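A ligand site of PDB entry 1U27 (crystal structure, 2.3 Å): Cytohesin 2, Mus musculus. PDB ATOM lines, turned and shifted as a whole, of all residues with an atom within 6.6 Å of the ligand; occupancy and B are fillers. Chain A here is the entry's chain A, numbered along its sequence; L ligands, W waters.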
ATOM      1  N   LYS A  19      19.491   0.021  24.178  1.00  0.00           N
ATOM      2  CA  LYS A  19      20.916   0.311  24.224  1.00  0.00           C
ATOM      3  C   LYS A  19      21.690  -0.747  23.464  1.00  0.00           C
ATOM      4  O   LYS A  19      21.359  -1.927  23.534  1.00  0.00           O
ATOM      5  CB  LYS A  19      21.377   0.349  25.671  1.00  0.00           C
ATOM      6  CG  LYS A  19      22.857   0.624  25.831  1.00  0.00           C
ATOM      7  CD  LYS A  19      23.230   0.773  27.304  1.00  0.00           C
ATOM      8  CE  LYS A  19      22.899  -0.495  28.085  1.00  0.00           C
ATOM      9  NZ  LYS A  19      23.668  -1.668  27.570  1.00  0.00           N
ATOM     10  N   LEU A  20      22.719  -0.345  22.733  1.00  0.00           N
ATOM     11  CA  LEU A  20      23.554  -1.272  21.974  1.00  0.00           C
ATOM     12  C   LEU A  20      24.731  -1.677  22.835  1.00  0.00           C
ATOM     13  O   LEU A  20      25.402  -0.819  23.425  1.00  0.00           O
ATOM     14  CB  LEU A  20      24.058  -0.597  20.709  1.00  0.00           C
ATOM     15  CG  LEU A  20      24.730  -1.563  19.753  1.00  0.00           C
ATOM     16  CD1 LEU A  20      23.654  -2.313  18.963  1.00  0.00           C
ATOM     17  CD2 LEU A  20      25.639  -0.784  18.805  1.00  0.00           C
ATOM     18  N   GLY A  21      25.019  -2.977  22.910  1.00  0.00           N
ATOM     19  CA  GLY A  21      26.096  -3.413  23.769  1.00  0.00           C
ATOM     20  C   GLY A  21      27.252  -4.251  23.243  1.00  0.00           C
ATOM     21  O   GLY A  21      28.256  -3.700  22.808  1.00  0.00           O
ATOM     22  N   GLY A  22      27.085  -5.582  23.320  1.00  0.00           N
ATOM     23  CA  GLY A  22      28.065  -6.583  22.897  1.00  0.00           C
ATOM     24  C   GLY A  22      29.367  -6.248  22.167  1.00  0.00           C
ATOM     25  O   GLY A  22      29.684  -5.103  21.849  1.00  0.00           O
ATOM     26  N   GLY A  23      30.139  -7.294  21.915  1.00  0.00           N
ATOM     27  CA  GLY A  23      31.400  -7.151  21.210  1.00  0.00           C
ATOM     28  C   GLY A  23      31.250  -7.400  19.723  1.00  0.00           C
ATOM     29  O   GLY A  23      30.782  -6.513  18.989  1.00  0.00           O
ATOM     30  N   VAL A  25      29.153  -9.379  18.013  1.00  0.00           N
ATOM     31  CA  VAL A  25      27.766  -9.253  17.606  1.00  0.00           C
ATOM     32  C   VAL A  25      27.150  -8.285  18.595  1.00  0.00           C
ATOM     33  O   VAL A  25      27.106  -8.565  19.787  1.00  0.00           O
ATOM     34  CB  VAL A  25      27.047 -10.605  17.670  1.00  0.00           C
ATOM     35  CG1 VAL A  25      25.625 -10.463  17.138  1.00  0.00           C
ATOM     36  CG2 VAL A  25      27.787 -11.628  16.842  1.00  0.00           C
ATOM     37  N   THR A  27      23.972  -6.448  20.114  1.00  0.00           N
ATOM     38  CA  THR A  27      22.518  -6.549  20.199  1.00  0.00           C
ATOM     39  C   THR A  27      21.902  -5.430  21.014  1.00  0.00           C
ATOM     40  O   THR A  27      22.508  -4.948  21.975  1.00  0.00           O
ATOM     41  CB  THR A  27      22.101  -7.896  20.818  1.00  0.00           C
ATOM     42  OG1 THR A  27      22.712  -8.032  22.098  1.00  0.00           O
ATOM     43  CG2 THR A  27      22.532  -9.056  19.926  1.00  0.00           C
ATOM     44  N   TRP A  28      20.693  -5.028  20.635  1.00  0.00           N
ATOM     45  CA  TRP A  28      19.976  -3.979  21.329  1.00  0.00           C
ATOM     46  C   TRP A  28      19.201  -4.536  22.514  1.00  0.00           C
ATOM     47  O   TRP A  28      18.474  -5.521  22.378  1.00  0.00           O
ATOM     48  CB  TRP A  28      18.986  -3.286  20.395  1.00  0.00           C
ATOM     49  CG  TRP A  28      19.632  -2.539  19.283  1.00  0.00           C
ATOM     50  CD1 TRP A  28      19.990  -3.020  18.059  1.00  0.00           C
ATOM     51  CD2 TRP A  28      20.005  -1.162  19.279  1.00  0.00           C
ATOM     52  NE1 TRP A  28      20.558  -2.039  17.298  1.00  0.00           N
ATOM     53  CE2 TRP A  28      20.573  -0.877  18.018  1.00  0.00           C
ATOM     54  CE3 TRP A  28      19.909  -0.122  20.215  1.00  0.00           C
ATOM     55  CZ2 TRP A  28      21.050   0.380  17.675  1.00  0.00           C
ATOM     56  CZ3 TRP A  28      20.372   1.136  19.873  1.00  0.00           C
ATOM     57  CH2 TRP A  28      20.938   1.375  18.616  1.00  0.00           C
ATOM     58  N   LYS A  29      19.352  -3.894  23.667  1.00  0.00           N
ATOM     59  CA  LYS A  29      18.638  -4.297  24.862  1.00  0.00           C
ATOM     60  C   LYS A  29      17.756  -3.148  25.358  1.00  0.00           C
ATOM     61  O   LYS A  29      18.115  -1.963  25.296  1.00  0.00           O
ATOM     62  CB  LYS A  29      19.637  -4.722  25.938  1.00  0.00           C
ATOM     63  CG  LYS A  29      20.336  -6.049  25.695  1.00  0.00           C
ATOM     64  CD  LYS A  29      19.346  -7.228  25.822  1.00  0.00           C
ATOM     65  CE  LYS A  29      20.071  -8.587  25.855  1.00  0.00           C
ATOM     66  NZ  LYS A  29      20.759  -8.930  24.577  1.00  0.00           N
ATOM     67  N   ARG A  31      16.318  -1.126  28.154  1.00  0.00           N
ATOM     68  CA  ARG A  31      16.697  -0.814  29.516  1.00  0.00           C
ATOM     69  C   ARG A  31      15.952   0.416  30.030  1.00  0.00           C
ATOM     70  O   ARG A  31      15.518   1.277  29.241  1.00  0.00           O
ATOM     71  CB  ARG A  31      18.205  -0.573  29.567  1.00  0.00           C
ATOM     72  CG  ARG A  31      19.035  -1.800  29.226  1.00  0.00           C
ATOM     73  CD  ARG A  31      19.059  -2.766  30.401  1.00  0.00           C
ATOM     74  NE  ARG A  31      19.754  -4.013  30.086  1.00  0.00           N
ATOM     75  CZ  ARG A  31      19.152  -5.121  29.647  1.00  0.00           C
ATOM     76  NH1 ARG A  31      17.822  -5.140  29.481  1.00  0.00           N
ATOM     77  NH2 ARG A  31      19.852  -6.204  29.384  1.00  0.00           N
ATOM     78  N   TYR A  42      20.980   2.832  34.287  1.00  0.00           N
ATOM     79  CA  TYR A  42      20.072   2.023  33.518  1.00  0.00           C
ATOM     80  C   TYR A  42      19.825   0.713  34.264  1.00  0.00           C
ATOM     81  O   TYR A  42      20.703   0.218  34.986  1.00  0.00           O
ATOM     82  CB  TYR A  42      20.588   1.817  32.088  1.00  0.00           C
ATOM     83  CG  TYR A  42      21.962   1.213  31.931  1.00  0.00           C
ATOM     84  CD1 TYR A  42      22.163  -0.160  31.935  1.00  0.00           C
ATOM     85  CD2 TYR A  42      23.060   2.033  31.671  1.00  0.00           C
ATOM     86  CE1 TYR A  42      23.412  -0.706  31.675  1.00  0.00           C
ATOM     87  CE2 TYR A  42      24.310   1.504  31.411  1.00  0.00           C
ATOM     88  CZ  TYR A  42      24.482   0.131  31.415  1.00  0.00           C
ATOM     89  OH  TYR A  42      25.732  -0.387  31.173  1.00  0.00           O
ATOM     90  N   GLU A  44      17.509  -3.268  34.284  1.00  0.00           N
ATOM     91  CA  GLU A  44      16.848  -4.279  33.472  1.00  0.00           C
ATOM     92  C   GLU A  44      15.352  -4.130  33.732  1.00  0.00           C
ATOM     93  O   GLU A  44      14.574  -4.057  32.786  1.00  0.00           O
ATOM     94  CB  GLU A  44      17.300  -5.681  33.852  1.00  0.00           C
ATOM     95  CG  GLU A  44      16.537  -6.801  33.154  1.00  0.00           C
ATOM     96  CD  GLU A  44      17.240  -8.156  33.232  1.00  0.00           C
ATOM     97  OE1 GLU A  44      17.702  -8.541  34.339  1.00  0.00           O
ATOM     98  OE2 GLU A  44      17.335  -8.823  32.174  1.00  0.00           O
ATOM     99  N   ARG A  52      22.038  -1.678  36.510  1.00  0.00           N
ATOM    100  CA  ARG A  52      22.796  -2.591  35.673  1.00  0.00           C
ATOM    101  C   ARG A  52      24.028  -1.818  35.169  1.00  0.00           C
ATOM    102  O   ARG A  52      25.036  -2.401  34.806  1.00  0.00           O
ATOM    103  CB  ARG A  52      21.951  -3.051  34.491  1.00  0.00           C
ATOM    104  CG  ARG A  52      22.675  -3.953  33.495  1.00  0.00           C
ATOM    105  CD  ARG A  52      23.180  -5.240  34.133  1.00  0.00           C
ATOM    106  NE  ARG A  52      22.108  -6.082  34.630  1.00  0.00           N
ATOM    107  CZ  ARG A  52      21.335  -6.855  33.860  1.00  0.00           C
ATOM    108  NH1 ARG A  52      21.518  -6.878  32.547  1.00  0.00           N
ATOM    109  NH2 ARG A  52      20.394  -7.606  34.405  1.00  0.00           N
ATOM    110  N   GLY A  53      23.925  -0.489  35.179  1.00  0.00           N
ATOM    111  CA  GLY A  53      25.025   0.349  34.732  1.00  0.00           C
ATOM    112  C   GLY A  53      24.909   1.792  35.199  1.00  0.00           C
ATOM    113  O   GLY A  53      23.802   2.326  35.313  1.00  0.00           O
ATOM    114  N   CYS A  89      30.552   2.145  35.444  1.00  0.00           N
ATOM    115  CA  CYS A  89      30.576   0.885  36.179  1.00  0.00           C
ATOM    116  C   CYS A  89      29.474   0.025  35.573  1.00  0.00           C
ATOM    117  O   CYS A  89      28.496   0.534  35.031  1.00  0.00           O
ATOM    118  CB  CYS A  89      30.301   1.131  37.662  1.00  0.00           C
ATOM    119  SG  CYS A  89      28.553   1.374  38.034  1.00  0.00           S
ATOM    120  N   LYS A  90      29.633  -1.295  35.662  1.00  0.00           N
ATOM    121  CA  LYS A  90      28.656  -2.228  35.135  1.00  0.00           C
ATOM    122  C   LYS A  90      28.539  -3.406  36.103  1.00  0.00           C
ATOM    123  O   LYS A  90      29.494  -3.717  36.805  1.00  0.00           O
ATOM    124  CB  LYS A  90      29.112  -2.725  33.755  1.00  0.00           C
ATOM    125  CG  LYS A  90      28.222  -3.790  33.166  1.00  0.00           C
ATOM    126  CD  LYS A  90      28.850  -4.436  31.945  1.00  0.00           C
ATOM    127  CE  LYS A  90      27.999  -5.597  31.473  1.00  0.00           C
ATOM    128  NZ  LYS A  90      28.591  -6.261  30.287  1.00  0.00           N
ATOM    129  N   THR A  91      27.385  -4.046  36.125  1.00  0.00           N
ATOM    130  CA  THR A  91      27.178  -5.193  37.017  1.00  0.00           C
ATOM    131  C   THR A  91      27.067  -6.497  36.234  1.00  0.00           C
ATOM    132  O   THR A  91      26.455  -6.550  35.174  1.00  0.00           O
ATOM    133  CB  THR A  91      25.914  -5.009  37.851  1.00  0.00           C
ATOM    134  OG1 THR A  91      26.089  -3.899  38.753  1.00  0.00           O
ATOM    135  CG2 THR A  91      25.612  -6.257  38.666  1.00  0.00           C
ATOM    136  N   GLU A  92      27.650  -7.561  36.781  1.00  0.00           N
ATOM    137  CA  GLU A  92      27.629  -8.872  36.141  1.00  0.00           C
ATOM    138  C   GLU A  92      26.611  -9.797  36.804  1.00  0.00           C
ATOM    139  O   GLU A  92      26.299  -9.633  37.975  1.00  0.00           O
ATOM    140  CB  GLU A  92      29.022  -9.515  36.207  1.00  0.00           C
ATOM    141  CG  GLU A  92      30.099  -8.770  35.429  1.00  0.00           C
ATOM    142  CD  GLU A  92      29.851  -8.783  33.929  1.00  0.00           C
ATOM    143  OE1 GLU A  92      28.773  -8.318  33.498  1.00  0.00           O
ATOM    144  OE2 GLU A  92      30.737  -9.261  33.188  1.00  0.00           O
ATOM    145  N   GLU A  99      34.462  -2.282  35.227  1.00  0.00           N
ATOM    146  CA  GLU A  99      34.474  -1.032  34.463  1.00  0.00           C
ATOM    147  C   GLU A  99      33.773  -1.237  33.123  1.00  0.00           C
ATOM    148  O   GLU A  99      33.844  -2.323  32.531  1.00  0.00           O
ATOM    149  CB  GLU A  99      35.899  -0.553  34.182  1.00  0.00           C
ATOM    150  CG  GLU A  99      36.687  -0.117  35.404  1.00  0.00           C
ATOM    151  CD  GLU A  99      37.696  -1.154  35.857  1.00  0.00           C
ATOM    152  OE1 GLU A  99      38.586  -1.507  35.051  1.00  0.00           O
ATOM    153  OE2 GLU A  99      37.596  -1.623  37.024  1.00  0.00           O
ATOM    154  N   GLY A 100      33.075  -0.199  32.663  1.00  0.00           N
ATOM    155  CA  GLY A 100      32.378  -0.293  31.396  1.00  0.00           C
ATOM    156  C   GLY A 100      33.394  -0.527  30.315  1.00  0.00           C
ATOM    157  O   GLY A 100      34.566  -0.173  30.479  1.00  0.00           O
ATOM    158  N   ASN A 101      32.954  -1.127  29.200  1.00  0.00           N
ATOM    159  CA  ASN A 101      33.856  -1.407  28.092  1.00  0.00           C
ATOM    160  C   ASN A 101      33.369  -0.743  26.802  1.00  0.00           C
ATOM    161  O   ASN A 101      33.555  -1.248  25.690  1.00  0.00           O
ATOM    162  CB  ASN A 101      33.989  -2.915  27.886  1.00  0.00           C
ATOM    163  CG  ASN A 101      35.134  -3.274  26.950  1.00  0.00           C
ATOM    164  OD1 ASN A 101      36.311  -2.968  27.236  1.00  0.00           O
ATOM    165  ND2 ASN A 101      34.814  -3.911  25.820  1.00  0.00           N
ATOM    166  N   HIS A 102      32.736   0.420  26.969  1.00  0.00           N
ATOM    167  CA  HIS A 102      32.223   1.184  25.842  1.00  0.00           C
ATOM    168  C   HIS A 102      33.155   2.324  25.459  1.00  0.00           C
ATOM    169  O   HIS A 102      33.850   2.898  26.304  1.00  0.00           O
ATOM    170  CB  HIS A 102      30.862   1.802  26.213  1.00  0.00           C
ATOM    171  CG  HIS A 102      29.693   0.895  26.001  1.00  0.00           C
ATOM    172  ND1 HIS A 102      28.929   0.918  24.839  1.00  0.00           N
ATOM    173  CD2 HIS A 102      29.140  -0.048  26.797  1.00  0.00           C
ATOM    174  CE1 HIS A 102      27.963   0.028  24.953  1.00  0.00           C
ATOM    175  NE2 HIS A 102      28.064  -0.569  26.125  1.00  0.00           N
ATOM    176  N   TYR A 105      28.198   5.020  23.691  1.00  0.00           N
ATOM    177  CA  TYR A 105      26.943   4.363  24.031  1.00  0.00           C
ATOM    178  C   TYR A 105      25.953   4.848  22.988  1.00  0.00           C
ATOM    179  O   TYR A 105      25.634   6.044  22.931  1.00  0.00           O
ATOM    180  CB  TYR A 105      26.454   4.750  25.420  1.00  0.00           C
ATOM    181  CG  TYR A 105      27.219   4.133  26.546  1.00  0.00           C
ATOM    182  CD1 TYR A 105      28.369   4.726  27.044  1.00  0.00           C
ATOM    183  CD2 TYR A 105      26.793   2.940  27.118  1.00  0.00           C
ATOM    184  CE1 TYR A 105      29.080   4.158  28.084  1.00  0.00           C
ATOM    185  CE2 TYR A 105      27.497   2.365  28.161  1.00  0.00           C
ATOM    186  CZ  TYR A 105      28.647   2.966  28.644  1.00  0.00           C
ATOM    187  OH  TYR A 105      29.359   2.402  29.691  1.00  0.00           O
HETATM  188  C1  LIG L   1      25.501  -7.964  26.595  1.00  0.00           C
HETATM  189  O1  LIG L   1      24.964  -8.712  25.490  1.00  0.00           O
HETATM  190  C2  LIG L   1      24.490  -6.858  27.013  1.00  0.00           C
HETATM  191  O2  LIG L   1      24.105  -6.079  25.864  1.00  0.00           O
HETATM  192  C3  LIG L   1      25.061  -5.936  28.082  1.00  0.00           C
HETATM  193  O3  LIG L   1      24.133  -4.903  28.356  1.00  0.00           O
HETATM  194  C4  LIG L   1      26.387  -5.298  27.659  1.00  0.00           C
HETATM  195  O4  LIG L   1      26.923  -4.580  28.771  1.00  0.00           O
HETATM  196  C5  LIG L   1      27.437  -6.321  27.177  1.00  0.00           C
HETATM  197  O5  LIG L   1      28.491  -5.590  26.526  1.00  0.00           O
HETATM  198  C6  LIG L   1      26.881  -7.383  26.194  1.00  0.00           C
HETATM  199  O6  LIG L   1      27.829  -8.455  26.084  1.00  0.00           O
HETATM  200  P1  LIG L   1      24.220 -10.153  25.691  1.00  0.00           P
HETATM  201  O7  LIG L   1      23.753 -10.574  24.338  1.00  0.00           O
HETATM  202  O8  LIG L   1      23.077  -9.934  26.630  1.00  0.00           O
HETATM  203  O9  LIG L   1      25.247 -11.083  26.267  1.00  0.00           O
HETATM  204  P2  LIG L   1      23.481  -4.730  29.820  1.00  0.00           P
HETATM  205  O10 LIG L   1      22.646  -3.510  29.756  1.00  0.00           O
HETATM  206  O11 LIG L   1      22.666  -5.947  30.072  1.00  0.00           O
HETATM  207  O12 LIG L   1      24.591  -4.601  30.790  1.00  0.00           O
HETATM  208  P3  LIG L   1      27.049  -2.965  28.789  1.00  0.00           P
HETATM  209  O13 LIG L   1      26.782  -2.498  27.407  1.00  0.00           O
HETATM  210  O14 LIG L   1      26.020  -2.484  29.742  1.00  0.00           O
HETATM  211  O15 LIG L   1      28.444  -2.655  29.245  1.00  0.00           O
HETATM  212  P4  LIG L   1      30.046  -5.795  26.896  1.00  0.00           P
HETATM  213  O16 LIG L   1      30.109  -6.660  28.115  1.00  0.00           O
HETATM  214  O17 LIG L   1      30.666  -6.448  25.703  1.00  0.00           O
HETATM  215  O18 LIG L   1      30.594  -4.429  27.142  1.00  0.00           O
HETATM  216  O   HOH W   1      21.688  -9.606  29.359  1.00  0.00           O
HETATM  217  O   HOH W   2      23.774  -8.427  30.492  1.00  0.00           O
HETATM  218  O   HOH W   3      22.720  -3.194  25.506  1.00  0.00           O
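The backbone carbonyl oxygen (O) of Tyr 42 is in hydrogen-bond range of the backbone NH (N) of Arg 52 (2.8 Å).
The side-chain amino group of Lys 90 lies within salt-bridge range of the side-chain carboxylate of Glu 92 (3.8 Å).
The backbone NH (N) of Gly 21 is in hydrogen-bond range of the backbone carbonyl oxygen (O) of Thr 27 (3.3 Å).
The side-chain amino group of Lys 29 lies within hydrogen-bond range of the side-chain hydroxyl of Thr 27 (3.3 Å).
The backbone NH (N) of Lys 19 sits at hydrogen-bond distance from the backbone carbonyl oxygen (O) of Lys 29.
The backbone NH (N) of Thr 91 lies within hydrogen-bond range of the backbone carbonyl oxygen (O) of Arg 52, 3.2 Å away.
NH2 of Arg 52 lies within salt-bridge range of OE1 of Glu 44.
The backbone carbonyl oxygen of Gly 53 is in hydrogen-bond range of the backbone NH of Tyr 42 (3.0 Å).
Gly 21 touches the ligand (C to O5, 3.8 Å).
Gly 22 touches the ligand.
Gly 23 touches the ligand (N to O17, 3.9 Å).
Thr 27 touches the ligand (OG1 to O7, 3.5 Å).
Asn 101 touches the ligand (CB to O18, 3.8 Å).
Hydrophobic or aromatic side chains within 4 Å of the ligand: Tyr 42 and His 102.
The nearest printed residue that does not touch the ligand is Leu 20 (4.5 Å).
An oxygen (O11) of the ligand is in salt-bridge range of the guanidinium group (NH1) of Arg 52 (2.9 Å).
A ring nitrogen (NE2) of His 102 sits at hydrogen-bond distance from an oxygen (O13) of the ligand (2.6 Å).
O8 of the ligand is in salt-bridge range of NZ of Lys 29, at 3.3 Å.
NZ of Lys 19 lies within salt-bridge range of O10 of the ligand, 3.0 Å away.
NZ of Lys 90 is in salt-bridge range of O16 of the ligand, 2.7 Å away.
An oxygen (O14) of the ligand is in hydrogen-bond range of the side-chain hydroxyl (OH) of Tyr 42 (2.6 Å).
The guanidinium group (NH2) of Arg 31 is in salt-bridge range of an oxygen (O11) of the ligand (2.9 Å).
Water W2 bridges an oxygen (O11) of the ligand (2.7 Å) and the guanidinium group of Arg 52 (3.4 Å).
Water W3 lies within hydrogen-bond range of the backbone carbonyl oxygen of Lys 19, an oxygen (O2) of the ligand and the backbone NH of Gly 21.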
